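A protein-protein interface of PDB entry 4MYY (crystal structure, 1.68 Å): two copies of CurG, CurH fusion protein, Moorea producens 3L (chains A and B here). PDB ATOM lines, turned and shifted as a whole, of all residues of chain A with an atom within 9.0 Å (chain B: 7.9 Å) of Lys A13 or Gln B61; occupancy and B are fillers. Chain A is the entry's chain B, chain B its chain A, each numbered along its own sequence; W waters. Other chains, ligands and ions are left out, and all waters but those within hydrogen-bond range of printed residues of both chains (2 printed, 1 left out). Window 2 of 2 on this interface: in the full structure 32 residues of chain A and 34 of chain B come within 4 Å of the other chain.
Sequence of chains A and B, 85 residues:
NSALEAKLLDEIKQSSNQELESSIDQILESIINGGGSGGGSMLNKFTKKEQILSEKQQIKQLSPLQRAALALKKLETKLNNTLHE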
ATOM      1  N   ALA A   6      -4.753 -21.744   6.869  1.00  0.00           N
ATOM      2  CA  ALA A   6      -6.094 -21.647   7.483  1.00  0.00           C
ATOM      3  C   ALA A   6      -6.869 -22.936   7.250  1.00  0.00           C
ATOM      4  O   ALA A   6      -7.534 -23.445   8.158  1.00  0.00           O
ATOM      5  CB  ALA A   6      -6.865 -20.474   6.911  1.00  0.00           C
ATOM      6  N   LYS A   7      -6.756 -23.467   6.033  1.00  0.00           N
ATOM      7  CA  LYS A   7      -7.415 -24.730   5.674  1.00  0.00           C
ATOM      8  C   LYS A   7      -6.936 -25.896   6.553  1.00  0.00           C
ATOM      9  O   LYS A   7      -7.739 -26.677   7.040  1.00  0.00           O
ATOM     10  CB  LYS A   7      -7.178 -25.052   4.183  1.00  0.00           C
ATOM     11  CG  LYS A   7      -7.958 -26.245   3.647  1.00  0.00           C
ATOM     12  CD  LYS A   7      -7.551 -26.457   2.182  1.00  0.00           C
ATOM     13  CE  LYS A   7      -8.352 -27.544   1.487  1.00  0.00           C
ATOM     14  NZ  LYS A   7      -9.770 -27.066   1.371  1.00  0.00           N
ATOM     15  N   LEU A   8      -5.619 -26.003   6.727  1.00  0.00           N
ATOM     16  CA  LEU A   8      -5.050 -27.072   7.531  1.00  0.00           C
ATOM     17  C   LEU A   8      -5.501 -26.978   8.987  1.00  0.00           C
ATOM     18  O   LEU A   8      -5.880 -27.979   9.577  1.00  0.00           O
ATOM     19  CB  LEU A   8      -3.532 -27.027   7.441  1.00  0.00           C
ATOM     20  CG  LEU A   8      -2.831 -28.025   8.364  1.00  0.00           C
ATOM     21  CD1 LEU A   8      -3.097 -29.451   7.886  1.00  0.00           C
ATOM     22  CD2 LEU A   8      -1.350 -27.699   8.433  1.00  0.00           C
ATOM     23  N   LEU A   9      -5.497 -25.781   9.541  1.00  0.00           N
ATOM     24  CA  LEU A   9      -5.914 -25.600  10.916  1.00  0.00           C
ATOM     25  C   LEU A   9      -7.372 -26.041  11.100  1.00  0.00           C
ATOM     26  O   LEU A   9      -7.682 -26.745  12.038  1.00  0.00           O
ATOM     27  CB  LEU A   9      -5.711 -24.162  11.341  1.00  0.00           C
ATOM     28  CG  LEU A   9      -5.523 -24.071  12.854  1.00  0.00           C
ATOM     29  CD1 LEU A   9      -4.478 -23.025  13.194  1.00  0.00           C
ATOM     30  CD2 LEU A   9      -6.864 -23.776  13.516  1.00  0.00           C
ATOM     31  N   ASP A  10      -8.239 -25.664  10.168  1.00  0.00           N
ATOM     32  CA  ASP A  10      -9.642 -26.068  10.212  1.00  0.00           C
ATOM     33  C   ASP A  10      -9.770 -27.590  10.110  1.00  0.00           C
ATOM     34  O   ASP A  10     -10.545 -28.194  10.852  1.00  0.00           O
ATOM     35  CB  ASP A  10     -10.430 -25.414   9.074  1.00  0.00           C
ATOM     36  CG  ASP A  10     -10.740 -23.940   9.332  1.00  0.00           C
ATOM     37  OD1 ASP A  10     -10.411 -23.419  10.418  1.00  0.00           O
ATOM     38  OD2 ASP A  10     -11.330 -23.302   8.426  1.00  0.00           O
ATOM     39  N   GLU A  11      -9.004 -28.212   9.218  1.00  0.00           N
ATOM     40  CA  GLU A  11      -9.053 -29.668   9.085  1.00  0.00           C
ATOM     41  C   GLU A  11      -8.629 -30.357  10.379  1.00  0.00           C
ATOM     42  O   GLU A  11      -9.325 -31.235  10.843  1.00  0.00           O
ATOM     43  CB  GLU A  11      -8.216 -30.154   7.915  1.00  0.00           C
ATOM     44  CG  GLU A  11      -8.834 -29.757   6.567  1.00  0.00           C
ATOM     45  CD  GLU A  11      -8.397 -30.660   5.434  1.00  0.00           C
ATOM     46  OE1 GLU A  11      -7.642 -31.637   5.678  1.00  0.00           O
ATOM     47  OE2 GLU A  11      -8.824 -30.394   4.280  1.00  0.00           O
ATOM     48  N   ILE A  12      -7.522 -29.903  10.975  1.00  0.00           N
ATOM     49  CA  ILE A  12      -7.035 -30.445  12.264  1.00  0.00           C
ATOM     50  C   ILE A  12      -8.106 -30.299  13.379  1.00  0.00           C
ATOM     51  O   ILE A  12      -8.392 -31.247  14.133  1.00  0.00           O
ATOM     52  CB  ILE A  12      -5.704 -29.783  12.652  1.00  0.00           C
ATOM     53  CG1 ILE A  12      -4.584 -30.292  11.729  1.00  0.00           C
ATOM     54  CG2 ILE A  12      -5.356 -30.065  14.134  1.00  0.00           C
ATOM     55  CD1 ILE A  12      -3.255 -29.596  11.924  1.00  0.00           C
ATOM     56  N   LYS A  13      -8.716 -29.125  13.469  1.00  0.00           N
ATOM     57  CA  LYS A  13      -9.746 -28.887  14.479  1.00  0.00           C
ATOM     58  C   LYS A  13     -10.940 -29.829  14.319  1.00  0.00           C
ATOM     59  O   LYS A  13     -11.545 -30.240  15.323  1.00  0.00           O
ATOM     60  CB  LYS A  13     -10.232 -27.425  14.433  1.00  0.00           C
ATOM     61  CG  LYS A  13     -11.004 -26.958  15.681  1.00  0.00           C
ATOM     62  CD  LYS A  13     -11.500 -25.529  15.498  1.00  0.00           C
ATOM     63  CE  LYS A  13     -12.054 -24.935  16.787  1.00  0.00           C
ATOM     64  NZ  LYS A  13     -13.117 -25.800  17.363  1.00  0.00           N
ATOM     65  N   GLN A  14     -11.286 -30.141  13.068  1.00  0.00           N
ATOM     66  CA  GLN A  14     -12.427 -30.993  12.763  1.00  0.00           C
ATOM     67  C   GLN A  14     -12.121 -32.471  12.867  1.00  0.00           C
ATOM     68  O   GLN A  14     -13.040 -33.275  12.888  1.00  0.00           O
ATOM     69  CB  GLN A  14     -12.959 -30.663  11.359  1.00  0.00           C
ATOM     70  CG  GLN A  14     -13.592 -29.291  11.305  1.00  0.00           C
ATOM     71  CD  GLN A  14     -13.710 -28.745   9.895  1.00  0.00           C
ATOM     72  OE1 GLN A  14     -13.775 -29.499   8.922  1.00  0.00           O
ATOM     73  NE2 GLN A  14     -13.725 -27.435   9.776  1.00  0.00           N
ATOM     74  N   SER A  15     -10.834 -32.819  12.995  1.00  0.00           N
ATOM     75  CA  SER A  15     -10.389 -34.219  12.946  1.00  0.00           C
ATOM     76  C   SER A  15     -10.619 -34.940  14.254  1.00  0.00           C
ATOM     77  O   SER A  15     -10.563 -34.338  15.319  1.00  0.00           O
ATOM     78  CB  SER A  15      -8.893 -34.293  12.637  1.00  0.00           C
ATOM     79  OG  SER A  15      -8.628 -33.873  11.325  1.00  0.00           O
ATOM     80  N   SER A  16     -10.823 -36.249  14.181  1.00  0.00           N
ATOM     81  CA  SER A  16     -10.950 -37.015  15.403  1.00  0.00           C
ATOM     82  C   SER A  16      -9.573 -37.238  16.013  1.00  0.00           C
ATOM     83  O   SER A  16      -8.579 -37.175  15.319  1.00  0.00           O
ATOM     84  CB  SER A  16     -11.634 -38.371  15.145  1.00  0.00           C
ATOM     85  OG  SER A  16     -10.758 -39.244  14.430  1.00  0.00           O
ATOM     86  N   ASN A  17      -9.534 -37.526  17.312  1.00  0.00           N
ATOM     87  CA  ASN A  17      -8.257 -37.879  17.924  1.00  0.00           C
ATOM     88  C   ASN A  17      -7.562 -39.066  17.274  1.00  0.00           C
ATOM     89  O   ASN A  17      -6.350 -39.023  17.110  1.00  0.00           O
ATOM     90  CB  ASN A  17      -8.378 -38.087  19.422  1.00  0.00           C
ATOM     91  CG  ASN A  17      -8.657 -36.803  20.165  1.00  0.00           C
ATOM     92  OD1 ASN A  17      -8.361 -35.721  19.679  1.00  0.00           O
ATOM     93  ND2 ASN A  17      -9.242 -36.916  21.359  1.00  0.00           N
ATOM     94  N   GLU A  19      -7.730 -39.980  14.169  1.00  0.00           N
ATOM     95  CA  GLU A  19      -7.163 -39.462  12.912  1.00  0.00           C
ATOM     96  C   GLU A  19      -5.826 -38.776  13.143  1.00  0.00           C
ATOM     97  O   GLU A  19      -4.874 -39.008  12.388  1.00  0.00           O
ATOM     98  CB  GLU A  19      -8.137 -38.506  12.209  1.00  0.00           C
ATOM     99  CG  GLU A  19      -9.225 -39.269  11.461  1.00  0.00           C
ATOM    100  CD  GLU A  19     -10.411 -38.425  11.025  1.00  0.00           C
ATOM    101  OE1 GLU A  19     -10.575 -37.281  11.482  1.00  0.00           O
ATOM    102  OE2 GLU A  19     -11.218 -38.948  10.210  1.00  0.00           O
ATOM    103  N   LEU A  20      -5.765 -37.905  14.155  1.00  0.00           N
ATOM    104  CA  LEU A  20      -4.538 -37.181  14.442  1.00  0.00           C
ATOM    105  C   LEU A  20      -3.466 -38.166  14.937  1.00  0.00           C
ATOM    106  O   LEU A  20      -2.294 -38.063  14.572  1.00  0.00           O
ATOM    107  CB  LEU A  20      -4.802 -36.126  15.522  1.00  0.00           C
ATOM    108  CG  LEU A  20      -5.741 -34.999  15.079  1.00  0.00           C
ATOM    109  CD1 LEU A  20      -5.905 -34.042  16.238  1.00  0.00           C
ATOM    110  CD2 LEU A  20      -5.237 -34.260  13.857  1.00  0.00           C
ATOM    111  N   GLU B  55      -3.571 -16.517  13.285  1.00  0.00           N
ATOM    112  CA  GLU B  55      -3.317 -17.930  13.530  1.00  0.00           C
ATOM    113  C   GLU B  55      -3.164 -18.201  15.020  1.00  0.00           C
ATOM    114  O   GLU B  55      -3.608 -19.256  15.510  1.00  0.00           O
ATOM    115  CB  GLU B  55      -2.092 -18.417  12.781  1.00  0.00           C
ATOM    116  CG  GLU B  55      -1.874 -19.908  12.971  1.00  0.00           C
ATOM    117  CD  GLU B  55      -0.981 -20.497  11.905  1.00  0.00           C
ATOM    118  OE1 GLU B  55      -0.250 -19.720  11.251  1.00  0.00           O
ATOM    119  OE2 GLU B  55      -1.021 -21.728  11.732  1.00  0.00           O
ATOM    120  N   LYS B  56      -2.538 -17.278  15.744  1.00  0.00           N
ATOM    121  CA  LYS B  56      -2.364 -17.461  17.179  1.00  0.00           C
ATOM    122  C   LYS B  56      -3.692 -17.478  17.932  1.00  0.00           C
ATOM    123  O   LYS B  56      -3.876 -18.245  18.888  1.00  0.00           O
ATOM    124  CB  LYS B  56      -1.413 -16.418  17.755  1.00  0.00           C
ATOM    125  CG  LYS B  56       0.036 -16.671  17.393  1.00  0.00           C
ATOM    126  CD  LYS B  56       0.934 -15.674  18.108  1.00  0.00           C
ATOM    127  CE  LYS B  56       2.386 -15.982  17.809  1.00  0.00           C
ATOM    128  NZ  LYS B  56       3.304 -15.143  18.626  1.00  0.00           N
ATOM    129  N   GLN B  57      -4.632 -16.660  17.476  1.00  0.00           N
ATOM    130  CA  GLN B  57      -5.986 -16.703  18.031  1.00  0.00           C
ATOM    131  C   GLN B  57      -6.636 -18.049  17.784  1.00  0.00           C
ATOM    132  O   GLN B  57      -7.292 -18.612  18.675  1.00  0.00           O
ATOM    133  CB  GLN B  57      -6.858 -15.574  17.459  1.00  0.00           C
ATOM    134  CG  GLN B  57      -6.535 -14.212  18.059  1.00  0.00           C
ATOM    135  CD  GLN B  57      -6.304 -14.281  19.567  1.00  0.00           C
ATOM    136  OE1 GLN B  57      -7.240 -14.473  20.350  1.00  0.00           O
ATOM    137  NE2 GLN B  57      -5.045 -14.133  19.978  1.00  0.00           N
ATOM    138  N   GLN B  58      -6.449 -18.587  16.586  1.00  0.00           N
ATOM    139  CA  GLN B  58      -7.089 -19.858  16.264  1.00  0.00           C
ATOM    140  C   GLN B  58      -6.473 -21.019  17.042  1.00  0.00           C
ATOM    141  O   GLN B  58      -7.194 -21.903  17.503  1.00  0.00           O
ATOM    142  CB  GLN B  58      -7.030 -20.122  14.767  1.00  0.00           C
ATOM    143  CG  GLN B  58      -7.753 -19.058  13.968  1.00  0.00           C
ATOM    144  CD  GLN B  58      -7.621 -19.302  12.499  1.00  0.00           C
ATOM    145  OE1 GLN B  58      -8.009 -20.356  12.013  1.00  0.00           O
ATOM    146  NE2 GLN B  58      -7.057 -18.336  11.778  1.00  0.00           N
ATOM    147  N   ILE B  59      -5.153 -20.988  17.230  1.00  0.00           N
ATOM    148  CA  ILE B  59      -4.447 -22.029  17.978  1.00  0.00           C
ATOM    149  C   ILE B  59      -4.986 -22.144  19.420  1.00  0.00           C
ATOM    150  O   ILE B  59      -5.038 -23.225  19.982  1.00  0.00           O
ATOM    151  CB  ILE B  59      -2.941 -21.748  17.939  1.00  0.00           C
ATOM    152  CG1 ILE B  59      -2.406 -22.139  16.557  1.00  0.00           C
ATOM    153  CG2 ILE B  59      -2.180 -22.479  19.031  1.00  0.00           C
ATOM    154  CD1 ILE B  59      -1.004 -21.603  16.264  1.00  0.00           C
ATOM    155  N   LYS B  60      -5.388 -21.014  19.999  1.00  0.00           N
ATOM    156  CA  LYS B  60      -5.969 -21.013  21.329  1.00  0.00           C
ATOM    157  C   LYS B  60      -7.188 -21.928  21.435  1.00  0.00           C
ATOM    158  O   LYS B  60      -7.451 -22.492  22.493  1.00  0.00           O
ATOM    159  CB  LYS B  60      -6.324 -19.580  21.741  1.00  0.00           C
ATOM    160  CG  LYS B  60      -5.106 -18.735  22.079  1.00  0.00           C
ATOM    161  CD  LYS B  60      -5.489 -17.275  22.297  1.00  0.00           C
ATOM    162  CE  LYS B  60      -4.324 -16.463  22.839  1.00  0.00           C
ATOM    163  NZ  LYS B  60      -4.713 -15.044  23.095  1.00  0.00           N
ATOM    164  N   GLN B  61      -7.908 -22.110  20.330  1.00  0.00           N
ATOM    165  CA  GLN B  61      -9.095 -22.971  20.326  1.00  0.00           C
ATOM    166  C   GLN B  61      -8.830 -24.465  20.132  1.00  0.00           C
ATOM    167  O   GLN B  61      -9.738 -25.290  20.270  1.00  0.00           O
ATOM    168  CB  GLN B  61     -10.100 -22.495  19.278  1.00  0.00           C
ATOM    169  CG  GLN B  61     -10.543 -21.055  19.452  1.00  0.00           C
ATOM    170  CD  GLN B  61     -11.630 -20.680  18.465  1.00  0.00           C
ATOM    171  OE1 GLN B  61     -11.602 -21.101  17.301  1.00  0.00           O
ATOM    172  NE2 GLN B  61     -12.597 -19.893  18.920  1.00  0.00           N
ATOM    173  N   LEU B  62      -7.581 -24.808  19.822  1.00  0.00           N
ATOM    174  CA  LEU B  62      -7.189 -26.187  19.569  1.00  0.00           C
ATOM    175  C   LEU B  62      -6.839 -26.920  20.861  1.00  0.00           C
ATOM    176  O   LEU B  62      -6.295 -26.314  21.792  1.00  0.00           O
ATOM    177  CB  LEU B  62      -5.960 -26.222  18.646  1.00  0.00           C
ATOM    178  CG  LEU B  62      -6.070 -25.615  17.238  1.00  0.00           C
ATOM    179  CD1 LEU B  62      -4.726 -25.815  16.524  1.00  0.00           C
ATOM    180  CD2 LEU B  62      -7.188 -26.259  16.437  1.00  0.00           C
ATOM    181  N   SER B  63      -7.108 -28.227  20.883  1.00  0.00           N
ATOM    182  CA  SER B  63      -6.690 -29.105  22.002  1.00  0.00           C
ATOM    183  C   SER B  63      -5.182 -29.350  21.960  1.00  0.00           C
ATOM    184  O   SER B  63      -4.563 -29.069  20.953  1.00  0.00           O
ATOM    185  CB  SER B  63      -7.353 -30.459  21.883  1.00  0.00           C
ATOM    186  OG  SER B  63      -6.893 -31.121  20.713  1.00  0.00           O
ATOM    187  N   PRO B  64      -4.614 -29.950  23.026  1.00  0.00           N
ATOM    188  CA  PRO B  64      -3.176 -30.206  23.010  1.00  0.00           C
ATOM    189  C   PRO B  64      -2.756 -31.120  21.857  1.00  0.00           C
ATOM    190  O   PRO B  64      -1.746 -30.862  21.194  1.00  0.00           O
ATOM    191  CB  PRO B  64      -2.947 -30.909  24.348  1.00  0.00           C
ATOM    192  CG  PRO B  64      -3.974 -30.308  25.245  1.00  0.00           C
ATOM    193  CD  PRO B  64      -5.200 -30.142  24.380  1.00  0.00           C
ATOM    194  N   GLN B  66      -4.307 -31.473  18.976  1.00  0.00           N
ATOM    195  CA  GLN B  66      -4.452 -30.707  17.730  1.00  0.00           C
ATOM    196  C   GLN B  66      -3.281 -29.758  17.523  1.00  0.00           C
ATOM    197  O   GLN B  66      -2.744 -29.670  16.406  1.00  0.00           O
ATOM    198  CB  GLN B  66      -5.773 -29.969  17.727  1.00  0.00           C
ATOM    199  CG  GLN B  66      -6.962 -30.901  17.571  1.00  0.00           C
ATOM    200  CD  GLN B  66      -8.288 -30.279  17.994  1.00  0.00           C
ATOM    201  OE1 GLN B  66      -8.375 -29.135  18.436  1.00  0.00           O
ATOM    202  NE2 GLN B  66      -9.339 -31.043  17.841  1.00  0.00           N
ATOM    203  N   ARG B  67      -2.886 -29.062  18.586  1.00  0.00           N
ATOM    204  CA  ARG B  67      -1.693 -28.206  18.555  1.00  0.00           C
ATOM    205  C   ARG B  67      -0.448 -29.026  18.144  1.00  0.00           C
ATOM    206  O   ARG B  67       0.377 -28.590  17.322  1.00  0.00           O
ATOM    207  CB  ARG B  67      -1.472 -27.542  19.918  1.00  0.00           C
ATOM    208  CG  ARG B  67      -2.550 -26.505  20.220  1.00  0.00           C
ATOM    209  CD  ARG B  67      -2.248 -25.759  21.493  1.00  0.00           C
ATOM    210  NE  ARG B  67      -3.376 -24.905  21.844  1.00  0.00           N
ATOM    211  CZ  ARG B  67      -3.571 -24.403  23.054  1.00  0.00           C
ATOM    212  NH1 ARG B  67      -2.701 -24.656  24.043  1.00  0.00           N
ATOM    213  NH2 ARG B  67      -4.639 -23.631  23.278  1.00  0.00           N
ATOM    214  N   ALA B  69      -0.339 -31.834  16.383  1.00  0.00           N
ATOM    215  CA  ALA B  69      -0.421 -32.211  14.978  1.00  0.00           C
ATOM    216  C   ALA B  69      -0.039 -31.038  14.060  1.00  0.00           C
ATOM    217  O   ALA B  69       0.688 -31.218  13.076  1.00  0.00           O
ATOM    218  CB  ALA B  69      -1.806 -32.686  14.660  1.00  0.00           C
HETATM  219  O   HOH W   1      -8.213 -33.444  21.015  1.00  0.00           O
HETATM  220  O   HOH W   2      -9.412 -34.104  17.779  1.00  0.00           O
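Printed residues of chain A within 4 Å of Gln B58: Leu A9 (3.9 Å). Ile B59 touches none of the printed residues of chain A. Printed residues of chain A within 4 Å of Leu B62: Leu A9 (3.8 Å) and Lys A13 (3.8 Å). The nearest printed residue of chain A that does not touch Ala B69 is Ile A12 (4.1 Å).
The backbone NH (N) of Ser B63 sits at hydrogen-bond distance from the side-chain amide oxygen (OE1) of Gln B66 (2.9 Å). O of Leu B62 lies within hydrogen-bond range of NE of Arg B67, at 3.2 Å.
Among the printed residues, merely in contact across the chains: Ile A12 with Gln B66, Leu A20 with Gln B66, Lys A13 with Leu B62, Leu A9 with Leu B62, Leu A20 with Ala B69, Leu A9 with Gln B58, Lys A13 with Gln B61 and Leu A9 with Glu B55.
Printed residues of chain B that touch a printed residue of chain A: Glu B55, Gln B58, Gln B61, Leu B62, Gln B66 and Ala B69. Hydrophobic or aromatic side chains of chain B within 4 Å of the printed part of chain A: Leu B62 and Ala B69. Hydrophobic or aromatic side chains of chain A within 4 Å of the printed part of chain B: Leu A9, Ile A12 and Leu A20. Among the printed residues, 9 pairs touch across the chains.
The side-chain amide nitrogen (NE2) of Gln B66 lies within hydrogen-bond range of the backbone carbonyl oxygen (O) of Lys A13 (3.4 Å).
No position is printed for both chains. Of the 9 pairs that touch across the chains among the printed residues, none has its exchanged pair printed and touching as well.
Water W1 bridges the side-chain amide oxygen (OD1) of Asn A17 (2.6 Å) and the side-chain hydroxyl (OG) of Ser B63 (2.7 Å). Water W2 lies within hydrogen-bond range of OD1 of Asn A17, O of Ser A15 and NE2 of Gln B66.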
